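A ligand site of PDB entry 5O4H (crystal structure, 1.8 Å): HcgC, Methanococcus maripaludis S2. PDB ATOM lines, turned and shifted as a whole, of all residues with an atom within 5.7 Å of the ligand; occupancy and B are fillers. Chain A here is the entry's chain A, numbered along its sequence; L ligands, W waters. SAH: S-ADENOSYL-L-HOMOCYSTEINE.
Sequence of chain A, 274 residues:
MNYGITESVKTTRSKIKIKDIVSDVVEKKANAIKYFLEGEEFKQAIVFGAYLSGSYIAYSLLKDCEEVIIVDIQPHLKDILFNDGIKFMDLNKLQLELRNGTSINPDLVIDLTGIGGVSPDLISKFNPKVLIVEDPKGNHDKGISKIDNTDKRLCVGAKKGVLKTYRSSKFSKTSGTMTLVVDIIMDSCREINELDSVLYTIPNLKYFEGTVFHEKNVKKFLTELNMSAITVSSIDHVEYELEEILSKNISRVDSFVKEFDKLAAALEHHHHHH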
ATOM      1  N   LYS A  29      -7.285  22.870   5.284  1.00  0.00           N
ATOM      2  CA  LYS A  29      -8.682  23.269   5.016  1.00  0.00           C
ATOM      3  C   LYS A  29      -9.627  22.358   5.811  1.00  0.00           C
ATOM      4  O   LYS A  29     -10.560  22.845   6.437  1.00  0.00           O
ATOM      5  CB  LYS A  29      -8.997  23.220   3.531  1.00  0.00           C
ATOM      6  CG  LYS A  29      -8.257  24.257   2.738  1.00  0.00           C
ATOM      7  CD  LYS A  29      -8.698  24.310   1.301  1.00  0.00           C
ATOM      8  CE  LYS A  29      -7.983  25.398   0.527  1.00  0.00           C
ATOM      9  NZ  LYS A  29      -8.595  25.611  -0.807  1.00  0.00           N
ATOM     10  N   PHE A  48     -20.451  20.595  -1.805  1.00  0.00           N
ATOM     11  CA  PHE A  48     -20.483  20.899  -3.234  1.00  0.00           C
ATOM     12  C   PHE A  48     -19.059  21.150  -3.703  1.00  0.00           C
ATOM     13  O   PHE A  48     -18.368  21.998  -3.135  1.00  0.00           O
ATOM     14  CB  PHE A  48     -21.315  22.139  -3.520  1.00  0.00           C
ATOM     15  CG  PHE A  48     -22.787  21.943  -3.326  1.00  0.00           C
ATOM     16  CD1 PHE A  48     -23.364  22.092  -2.080  1.00  0.00           C
ATOM     17  CD2 PHE A  48     -23.600  21.618  -4.409  1.00  0.00           C
ATOM     18  CE1 PHE A  48     -24.727  21.922  -1.907  1.00  0.00           C
ATOM     19  CE2 PHE A  48     -24.954  21.451  -4.240  1.00  0.00           C
ATOM     20  CZ  PHE A  48     -25.515  21.594  -2.992  1.00  0.00           C
ATOM     21  N   GLY A  49     -18.633  20.422  -4.729  1.00  0.00           N
ATOM     22  CA  GLY A  49     -17.286  20.572  -5.297  1.00  0.00           C
ATOM     23  C   GLY A  49     -16.303  19.525  -4.825  1.00  0.00           C
ATOM     24  O   GLY A  49     -15.730  19.654  -3.744  1.00  0.00           O
ATOM     25  N   ALA A  50     -16.101  18.469  -5.640  1.00  0.00           N
ATOM     26  CA  ALA A  50     -15.201  17.366  -5.315  1.00  0.00           C
ATOM     27  C   ALA A  50     -13.734  17.704  -5.520  1.00  0.00           C
ATOM     28  O   ALA A  50     -12.904  17.261  -4.746  1.00  0.00           O
ATOM     29  CB  ALA A  50     -15.568  16.155  -6.141  1.00  0.00           C
ATOM     30  N   TYR A  51     -13.410  18.467  -6.551  1.00  0.00           N
ATOM     31  CA  TYR A  51     -12.036  18.832  -6.829  1.00  0.00           C
ATOM     32  C   TYR A  51     -11.730  20.182  -6.133  1.00  0.00           C
ATOM     33  O   TYR A  51     -12.544  21.097  -6.244  1.00  0.00           O
ATOM     34  CB  TYR A  51     -11.811  18.949  -8.329  1.00  0.00           C
ATOM     35  CG  TYR A  51     -10.497  19.584  -8.744  1.00  0.00           C
ATOM     36  CD1 TYR A  51     -10.400  20.960  -8.904  1.00  0.00           C
ATOM     37  CD2 TYR A  51      -9.385  18.811  -9.025  1.00  0.00           C
ATOM     38  CE1 TYR A  51      -9.202  21.557  -9.296  1.00  0.00           C
ATOM     39  CE2 TYR A  51      -8.191  19.391  -9.439  1.00  0.00           C
ATOM     40  CZ  TYR A  51      -8.107  20.759  -9.583  1.00  0.00           C
ATOM     41  OH  TYR A  51      -6.905  21.292  -9.974  1.00  0.00           O
ATOM     42  N   LEU A  52     -10.595  20.370  -5.460  1.00  0.00           N
ATOM     43  CA  LEU A  52      -9.519  19.412  -5.210  1.00  0.00           C
ATOM     44  C   LEU A  52      -9.604  18.987  -3.735  1.00  0.00           C
ATOM     45  O   LEU A  52      -9.420  17.811  -3.435  1.00  0.00           O
ATOM     46  CB  LEU A  52      -8.162  20.049  -5.510  1.00  0.00           C
ATOM     47  CG  LEU A  52      -6.913  19.161  -5.332  1.00  0.00           C
ATOM     48  CD1 LEU A  52      -7.092  17.795  -5.926  1.00  0.00           C
ATOM     49  CD2 LEU A  52      -5.703  19.840  -5.924  1.00  0.00           C
ATOM     50  N   SER A  53      -9.882  19.917  -2.817  1.00  0.00           N
ATOM     51  CA  SER A  53      -9.975  19.577  -1.384  1.00  0.00           C
ATOM     52  C   SER A  53     -11.250  18.900  -0.974  1.00  0.00           C
ATOM     53  O   SER A  53     -11.281  18.367   0.102  1.00  0.00           O
ATOM     54  CB  SER A  53      -9.940  20.812  -0.513  1.00  0.00           C
ATOM     55  OG  SER A  53      -9.057  21.801  -1.001  1.00  0.00           O
ATOM     56  N   GLY A  54     -12.296  18.967  -1.808  1.00  0.00           N
ATOM     57  CA  GLY A  54     -13.578  18.377  -1.485  1.00  0.00           C
ATOM     58  C   GLY A  54     -13.537  16.914  -1.113  1.00  0.00           C
ATOM     59  O   GLY A  54     -14.190  16.521  -0.152  1.00  0.00           O
ATOM     60  N   VAL A  71     -21.427  16.571  -4.040  1.00  0.00           N
ATOM     61  CA  VAL A  71     -22.196  16.951  -5.210  1.00  0.00           C
ATOM     62  C   VAL A  71     -21.251  17.623  -6.187  1.00  0.00           C
ATOM     63  O   VAL A  71     -20.509  18.543  -5.819  1.00  0.00           O
ATOM     64  CB  VAL A  71     -23.405  17.859  -4.892  1.00  0.00           C
ATOM     65  CG1 VAL A  71     -24.122  18.265  -6.178  1.00  0.00           C
ATOM     66  CG2 VAL A  71     -24.365  17.158  -3.945  1.00  0.00           C
ATOM     67  N   ASP A  72     -21.274  17.192  -7.446  1.00  0.00           N
ATOM     68  CA  ASP A  72     -20.425  17.826  -8.457  1.00  0.00           C
ATOM     69  C   ASP A  72     -21.175  17.895  -9.759  1.00  0.00           C
ATOM     70  O   ASP A  72     -21.932  16.994 -10.093  1.00  0.00           O
ATOM     71  CB  ASP A  72     -19.064  17.163  -8.617  1.00  0.00           C
ATOM     72  CG  ASP A  72     -18.033  18.165  -9.080  1.00  0.00           C
ATOM     73  OD1 ASP A  72     -18.114  18.606 -10.246  1.00  0.00           O
ATOM     74  OD2 ASP A  72     -17.177  18.549  -8.275  1.00  0.00           O
ATOM     75  N   ILE A  73     -20.956  18.982 -10.483  1.00  0.00           N
ATOM     76  CA  ILE A  73     -21.567  19.220 -11.792  1.00  0.00           C
ATOM     77  C   ILE A  73     -20.930  18.261 -12.826  1.00  0.00           C
ATOM     78  O   ILE A  73     -21.547  17.995 -13.846  1.00  0.00           O
ATOM     79  CB  ILE A  73     -21.437  20.721 -12.170  1.00  0.00           C
ATOM     80  CG1 ILE A  73     -22.380  21.107 -13.303  1.00  0.00           C
ATOM     81  CG2 ILE A  73     -19.998  21.126 -12.523  1.00  0.00           C
ATOM     82  CD1 ILE A  73     -22.621  22.629 -13.399  1.00  0.00           C
ATOM     83  N   GLN A  74     -19.707  17.753 -12.571  1.00  0.00           N
ATOM     84  CA  GLN A  74     -19.000  16.825 -13.456  1.00  0.00           C
ATOM     85  C   GLN A  74     -19.164  15.402 -12.934  1.00  0.00           C
ATOM     86  O   GLN A  74     -18.534  15.075 -11.934  1.00  0.00           O
ATOM     87  CB  GLN A  74     -17.488  17.152 -13.505  1.00  0.00           C
ATOM     88  CG  GLN A  74     -17.160  18.550 -14.004  1.00  0.00           C
ATOM     89  CD  GLN A  74     -17.226  18.714 -15.502  1.00  0.00           C
ATOM     90  OE1 GLN A  74     -17.282  17.734 -16.269  1.00  0.00           O
ATOM     91  NE2 GLN A  74     -17.162  19.948 -15.950  1.00  0.00           N
ATOM     92  N   LEU A  77     -16.073  13.128 -11.730  1.00  0.00           N
ATOM     93  CA  LEU A  77     -15.364  13.428 -10.514  1.00  0.00           C
ATOM     94  C   LEU A  77     -15.687  12.442  -9.378  1.00  0.00           C
ATOM     95  O   LEU A  77     -15.087  12.564  -8.322  1.00  0.00           O
ATOM     96  CB  LEU A  77     -15.504  14.897 -10.100  1.00  0.00           C
ATOM     97  CG  LEU A  77     -14.687  15.827 -10.973  1.00  0.00           C
ATOM     98  CD1 LEU A  77     -14.844  17.237 -10.523  1.00  0.00           C
ATOM     99  CD2 LEU A  77     -13.195  15.483 -10.954  1.00  0.00           C
ATOM    100  N   LEU A  91     -24.936  17.183  -9.915  1.00  0.00           N
ATOM    101  CA  LEU A  91     -25.796  18.332  -9.649  1.00  0.00           C
ATOM    102  C   LEU A  91     -27.232  18.161 -10.146  1.00  0.00           C
ATOM    103  O   LEU A  91     -28.158  18.529  -9.437  1.00  0.00           O
ATOM    104  CB  LEU A  91     -25.153  19.601 -10.221  1.00  0.00           C
ATOM    105  CG  LEU A  91     -25.895  20.934  -9.993  1.00  0.00           C
ATOM    106  CD1 LEU A  91     -25.979  21.274  -8.517  1.00  0.00           C
ATOM    107  CD2 LEU A  91     -25.226  22.038 -10.751  1.00  0.00           C
ATOM    108  N   LEU A 112     -17.731  24.411  -1.694  1.00  0.00           N
ATOM    109  CA  LEU A 112     -16.314  24.569  -2.034  1.00  0.00           C
ATOM    110  C   LEU A 112     -16.142  24.866  -3.539  1.00  0.00           C
ATOM    111  O   LEU A 112     -15.033  24.763  -4.058  1.00  0.00           O
ATOM    112  CB  LEU A 112     -15.592  23.235  -1.714  1.00  0.00           C
ATOM    113  CG  LEU A 112     -15.749  22.670  -0.311  1.00  0.00           C
ATOM    114  CD1 LEU A 112     -15.105  21.324  -0.213  1.00  0.00           C
ATOM    115  CD2 LEU A 112     -15.153  23.596   0.719  1.00  0.00           C
ATOM    116  N   THR A 113     -17.202  25.244  -4.232  1.00  0.00           N
ATOM    117  CA  THR A 113     -17.154  25.478  -5.679  1.00  0.00           C
ATOM    118  C   THR A 113     -16.435  26.742  -6.121  1.00  0.00           C
ATOM    119  O   THR A 113     -15.948  26.757  -7.239  1.00  0.00           O
ATOM    120  CB  THR A 113     -18.530  25.403  -6.264  1.00  0.00           C
ATOM    121  OG1 THR A 113     -19.350  26.465  -5.768  1.00  0.00           O
ATOM    122  CG2 THR A 113     -19.173  24.047  -5.989  1.00  0.00           C
ATOM    123  N   GLY A 114     -16.379  27.768  -5.290  1.00  0.00           N
ATOM    124  CA  GLY A 114     -15.684  28.978  -5.680  1.00  0.00           C
ATOM    125  C   GLY A 114     -16.320  29.771  -6.808  1.00  0.00           C
ATOM    126  O   GLY A 114     -17.530  29.757  -6.994  1.00  0.00           O
ATOM    127  N   GLY A 116     -17.872  31.178 -10.024  1.00  0.00           N
ATOM    128  CA  GLY A 116     -18.792  30.623 -11.012  1.00  0.00           C
ATOM    129  C   GLY A 116     -19.417  29.289 -10.607  1.00  0.00           C
ATOM    130  O   GLY A 116     -19.910  28.546 -11.461  1.00  0.00           O
ATOM    131  N   GLY A 117     -19.399  28.999  -9.318  1.00  0.00           N
ATOM    132  CA  GLY A 117     -19.926  27.769  -8.768  1.00  0.00           C
ATOM    133  C   GLY A 117     -21.403  27.729  -8.448  1.00  0.00           C
ATOM    134  O   GLY A 117     -22.218  28.237  -9.209  1.00  0.00           O
ATOM    135  N   VAL A 118     -21.733  27.134  -7.333  1.00  0.00           N
ATOM    136  CA  VAL A 118     -23.120  26.988  -6.893  1.00  0.00           C
ATOM    137  C   VAL A 118     -23.809  28.339  -6.714  1.00  0.00           C
ATOM    138  O   VAL A 118     -23.202  29.299  -6.246  1.00  0.00           O
ATOM    139  CB  VAL A 118     -23.201  26.108  -5.632  1.00  0.00           C
ATOM    140  CG1 VAL A 118     -22.784  26.866  -4.379  1.00  0.00           C
ATOM    141  CG2 VAL A 118     -24.584  25.547  -5.468  1.00  0.00           C
ATOM    142  N   SER A 119     -25.094  28.401  -7.089  1.00  0.00           N
ATOM    143  CA  SER A 119     -25.835  29.641  -6.989  1.00  0.00           C
ATOM    144  C   SER A 119     -26.432  29.837  -5.623  1.00  0.00           C
ATOM    145  O   SER A 119     -26.848  28.870  -4.983  1.00  0.00           O
ATOM    146  CB  SER A 119     -26.995  29.649  -7.988  1.00  0.00           C
ATOM    147  OG  SER A 119     -27.957  28.692  -7.613  1.00  0.00           O
ATOM    148  N   LEU A 122     -29.722  27.918  -5.202  1.00  0.00           N
ATOM    149  CA  LEU A 122     -29.704  26.507  -4.810  1.00  0.00           C
ATOM    150  C   LEU A 122     -29.427  26.403  -3.315  1.00  0.00           C
ATOM    151  O   LEU A 122     -30.081  25.627  -2.635  1.00  0.00           O
ATOM    152  CB  LEU A 122     -28.671  25.698  -5.604  1.00  0.00           C
ATOM    153  CG  LEU A 122     -28.486  24.215  -5.174  1.00  0.00           C
ATOM    154  CD1 LEU A 122     -29.801  23.455  -5.188  1.00  0.00           C
ATOM    155  CD2 LEU A 122     -27.527  23.505  -6.085  1.00  0.00           C
ATOM    156  N   GLU A 134     -16.780  28.369   1.048  1.00  0.00           N
ATOM    157  CA  GLU A 134     -15.367  28.663   0.866  1.00  0.00           C
ATOM    158  C   GLU A 134     -15.250  29.946   0.075  1.00  0.00           C
ATOM    159  O   GLU A 134     -15.865  30.089  -0.981  1.00  0.00           O
ATOM    160  CB  GLU A 134     -14.626  27.547   0.108  1.00  0.00           C
ATOM    161  CG  GLU A 134     -13.132  27.807   0.014  1.00  0.00           C
ATOM    162  CD  GLU A 134     -12.272  26.640  -0.414  1.00  0.00           C
ATOM    163  OE1 GLU A 134     -12.807  25.666  -0.992  1.00  0.00           O
ATOM    164  OE2 GLU A 134     -11.028  26.754  -0.244  1.00  0.00           O
ATOM    165  N   SER A 175      -7.629  31.305  -3.085  1.00  0.00           N
ATOM    166  CA  SER A 175      -7.462  30.347  -1.991  1.00  0.00           C
ATOM    167  C   SER A 175      -7.564  28.913  -2.533  1.00  0.00           C
ATOM    168  O   SER A 175      -7.537  27.971  -1.739  1.00  0.00           O
ATOM    169  CB  SER A 175      -8.550  30.558  -0.965  1.00  0.00           C
ATOM    170  OG  SER A 175      -9.777  30.335  -1.639  1.00  0.00           O
ATOM    171  N   GLY A 176      -7.700  28.752  -3.866  1.00  0.00           N
ATOM    172  CA  GLY A 176      -7.817  27.433  -4.488  1.00  0.00           C
ATOM    173  C   GLY A 176      -6.623  26.563  -4.163  1.00  0.00           C
ATOM    174  O   GLY A 176      -5.501  27.029  -4.211  1.00  0.00           O
ATOM    175  N   THR A 177      -6.853  25.300  -3.812  1.00  0.00           N
ATOM    176  CA  THR A 177      -5.773  24.385  -3.444  1.00  0.00           C
ATOM    177  C   THR A 177      -4.667  24.324  -4.448  1.00  0.00           C
ATOM    178  O   THR A 177      -3.509  24.513  -4.096  1.00  0.00           O
ATOM    179  CB  THR A 177      -6.332  22.978  -3.210  1.00  0.00           C
ATOM    180  OG1 THR A 177      -7.358  23.038  -2.238  1.00  0.00           O
ATOM    181  CG2 THR A 177      -5.276  21.972  -2.773  1.00  0.00           C
ATOM    182  N   MET A 178      -4.977  23.994  -5.699  1.00  0.00           N
ATOM    183  CA  MET A 178      -3.927  23.870  -6.727  1.00  0.00           C
ATOM    184  C   MET A 178      -3.185  25.183  -6.981  1.00  0.00           C
ATOM    185  O   MET A 178      -1.972  25.144  -7.204  1.00  0.00           O
ATOM    186  CB  MET A 178      -4.510  23.216  -8.013  1.00  0.00           C
ATOM    187  CG  MET A 178      -3.503  22.276  -8.753  1.00  0.00           C
ATOM    188  SD  MET A 178      -2.853  20.811  -7.783  1.00  0.00           S
ATOM    189  CE  MET A 178      -1.192  21.026  -8.086  1.00  0.00           C
ATOM    190  N   PHE A 213     -10.290  18.071 -15.880  1.00  0.00           N
ATOM    191  CA  PHE A 213     -11.517  18.530 -16.530  1.00  0.00           C
ATOM    192  C   PHE A 213     -11.653  18.405 -18.029  1.00  0.00           C
ATOM    193  O   PHE A 213     -12.797  18.385 -18.503  1.00  0.00           O
ATOM    194  CB  PHE A 213     -11.723  20.010 -16.147  1.00  0.00           C
ATOM    195  CG  PHE A 213     -11.988  20.128 -14.673  1.00  0.00           C
ATOM    196  CD1 PHE A 213     -13.261  19.898 -14.168  1.00  0.00           C
ATOM    197  CD2 PHE A 213     -10.958  20.409 -13.793  1.00  0.00           C
ATOM    198  CE1 PHE A 213     -13.490  19.948 -12.802  1.00  0.00           C
ATOM    199  CE2 PHE A 213     -11.200  20.489 -12.428  1.00  0.00           C
ATOM    200  CZ  PHE A 213     -12.467  20.254 -11.938  1.00  0.00           C
HETATM  201  N   SAH L   1     -12.301  25.259  -3.814  1.00  0.00           N
HETATM  202  CA  SAH L   1     -11.661  24.075  -4.469  1.00  0.00           C
HETATM  203  CB  SAH L   1     -11.606  24.290  -5.991  1.00  0.00           C
HETATM  204  CG  SAH L   1     -13.004  24.350  -6.580  1.00  0.00           C
HETATM  205  SD  SAH L   1     -13.041  24.003  -8.335  1.00  0.00           S
HETATM  206  C   SAH L   1     -10.249  23.874  -3.976  1.00  0.00           C
HETATM  207  O   SAH L   1      -9.674  22.796  -4.204  1.00  0.00           O
HETATM  208  OXT SAH L   1      -9.679  24.799  -3.344  1.00  0.00           O
HETATM  209  C5' SAH L   1     -14.774  23.894  -8.584  1.00  0.00           C
HETATM  210  C4' SAH L   1     -15.245  22.459  -8.241  1.00  0.00           C
HETATM  211  O4' SAH L   1     -16.673  22.529  -8.069  1.00  0.00           O
HETATM  212  C3' SAH L   1     -15.051  21.469  -9.408  1.00  0.00           C
HETATM  213  O3' SAH L   1     -15.046  20.142  -8.872  1.00  0.00           O
HETATM  214  C2' SAH L   1     -16.310  21.689 -10.233  1.00  0.00           C
HETATM  215  O2' SAH L   1     -16.651  20.589 -11.082  1.00  0.00           O
HETATM  216  C1' SAH L   1     -17.358  21.850  -9.144  1.00  0.00           C
HETATM  217  N9  SAH L   1     -18.512  22.709  -9.469  1.00  0.00           N
HETATM  218  C8  SAH L   1     -18.535  23.868 -10.189  1.00  0.00           C
HETATM  219  N7  SAH L   1     -19.793  24.378 -10.220  1.00  0.00           N
HETATM  220  C5  SAH L   1     -20.567  23.545  -9.494  1.00  0.00           C
HETATM  221  C6  SAH L   1     -21.985  23.501  -9.103  1.00  0.00           C
HETATM  222  N6  SAH L   1     -22.830  24.466  -9.534  1.00  0.00           N
HETATM  223  N1  SAH L   1     -22.414  22.470  -8.327  1.00  0.00           N
HETATM  224  C2  SAH L   1     -21.579  21.493  -7.904  1.00  0.00           C
HETATM  225  N3  SAH L   1     -20.271  21.454  -8.225  1.00  0.00           N
HETATM  226  C4  SAH L   1     -19.727  22.441  -9.000  1.00  0.00           C
HETATM  227  O   HOH W   1     -12.336  23.109  -1.608  1.00  0.00           O
HETATM  228  O   HOH W   2     -21.642  26.206 -11.742  1.00  0.00           O
HETATM  229  O   HOH W   3     -25.944  25.798  -9.014  1.00  0.00           O
HETATM  230  O   HOH W   4     -11.030  28.181  -2.930  1.00  0.00           O
HETATM  231  O   HOH W   5     -16.205  25.477 -12.035  1.00  0.00           O
HETATM  232  O   HOH W   6      -7.903  23.400  -6.505  1.00  0.00           O
HETATM  233  O   HOH W   7     -16.711  21.945 -13.654  1.00  0.00           O
HETATM  234  O   HOH W   8     -11.594  27.967  -5.470  1.00  0.00           O
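An oxygen (O2') of the ligand is in hydrogen-bond range of the side-chain carboxylate (OD1) of Asp 72 (2.6 Å).
A nitrogen (N) of the ligand is in hydrogen-bond range of the backbone carbonyl oxygen (O) of Leu 112, 2.8 Å away.
NZ of Lys 29 is in salt-bridge range of OXT of the ligand (2.9 Å).
The backbone NH (N) of Leu 52 lies within hydrogen-bond range of an oxygen (O) of the ligand, at 2.9 Å.
The side-chain carboxylate (OE1) of Glu 134 lies within salt-bridge range of a nitrogen (N) of the ligand (2.9 Å).
The backbone NH (N) of Thr 177 lies within hydrogen-bond range of an oxygen (OXT) of the ligand, at 2.9 Å.
The side-chain hydroxyl (OG1) of Thr 177 is in hydrogen-bond range of an oxygen (O) of the ligand (3.0 Å).
O of the ligand lies within hydrogen-bond range of N of Ser 53, 3.2 Å away.
The side-chain hydroxyl of Ser 53 lies within hydrogen-bond range of an oxygen (O) of the ligand (3.4 Å).
N of Tyr 51 lies within hydrogen-bond range of O3' of the ligand (3.3 Å).
The backbone NH (N) of Ile 73 sits at hydrogen-bond distance from a nitrogen (N3) of the ligand, at 3.4 Å.
The backbone NH (N) of Gln 74 is in hydrogen-bond range of the side-chain carboxylate (OD1) of Asp 72 (2.9 Å).
O of Asp 72 sits at hydrogen-bond distance from N of Leu 91 (3.0 Å).
The side-chain carboxylate (OD2) of Asp 72 sits at hydrogen-bond distance from the backbone NH (N) of Ala 50 (2.8 Å).
The side-chain amino group of Lys 29 is in salt-bridge range of the side-chain carboxylate of Glu 134.
The side-chain amino group (NZ) of Lys 29 is in hydrogen-bond range of the backbone carbonyl oxygen (O) of Ser 175.
The side-chain hydroxyl of Thr 177 sits at hydrogen-bond distance from the side-chain hydroxyl of Ser 53 (2.4 Å).
OG1 of Thr 113 lies within hydrogen-bond range of N of Val 118 (2.9 Å).
The backbone NH of Gly 49 is in hydrogen-bond range of the backbone carbonyl oxygen of Val 71 (2.9 Å).
Gly 49 touches the ligand.
Ala 50 touches the ligand.
Val 71 touches the ligand.
Gln 74 touches the ligand.
CD1 of Leu 77 touches O3' of the ligand (3.3 Å).
Leu 91 touches the ligand.
O of Thr 113 touches C5' of the ligand (3.4 Å).
CA of Gly 117 touches N7 of the ligand (3.7 Å).
N of Val 118 touches N6 of the ligand, 3.6 Å away.
CA of Gly 176 touches OXT of the ligand (3.4 Å).
Phe 213 touches the ligand.
20 residues have an atom within 4 Å of the ligand: Lys 29, Gly 49, Ala 50, Tyr 51, Leu 52, Ser 53, Val 71, Asp 72, Ile 73, Gln 74, Leu 77, Leu 91, Leu 112, Thr 113, Gly 117, Val 118, Glu 134, Gly 176, Thr 177 and Phe 213.
Water W7 lies within hydrogen-bond range of O2' of the ligand (2.9 Å) and NE2 of Gln 74 (3.1 Å).
Water W6 lies within hydrogen-bond range of O of the ligand (3.0 Å), N of Met 178 (3.1 Å) and N of Thr 177 (3.5 Å).
Water W1 bridges the side-chain carboxylate of Glu 134 (2.7 Å) and a nitrogen (N) of the ligand (3.1 Å).
Water W4 lies within hydrogen-bond range of the side-chain hydroxyl of Ser 175 (2.8 Å), the side-chain carboxylate of Glu 134 (3.0 Å) and a nitrogen (N) of the ligand (3.3 Å).
Water W3 bridges N of Ser 119 (3.3 Å) and N6 of the ligand (3.4 Å).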
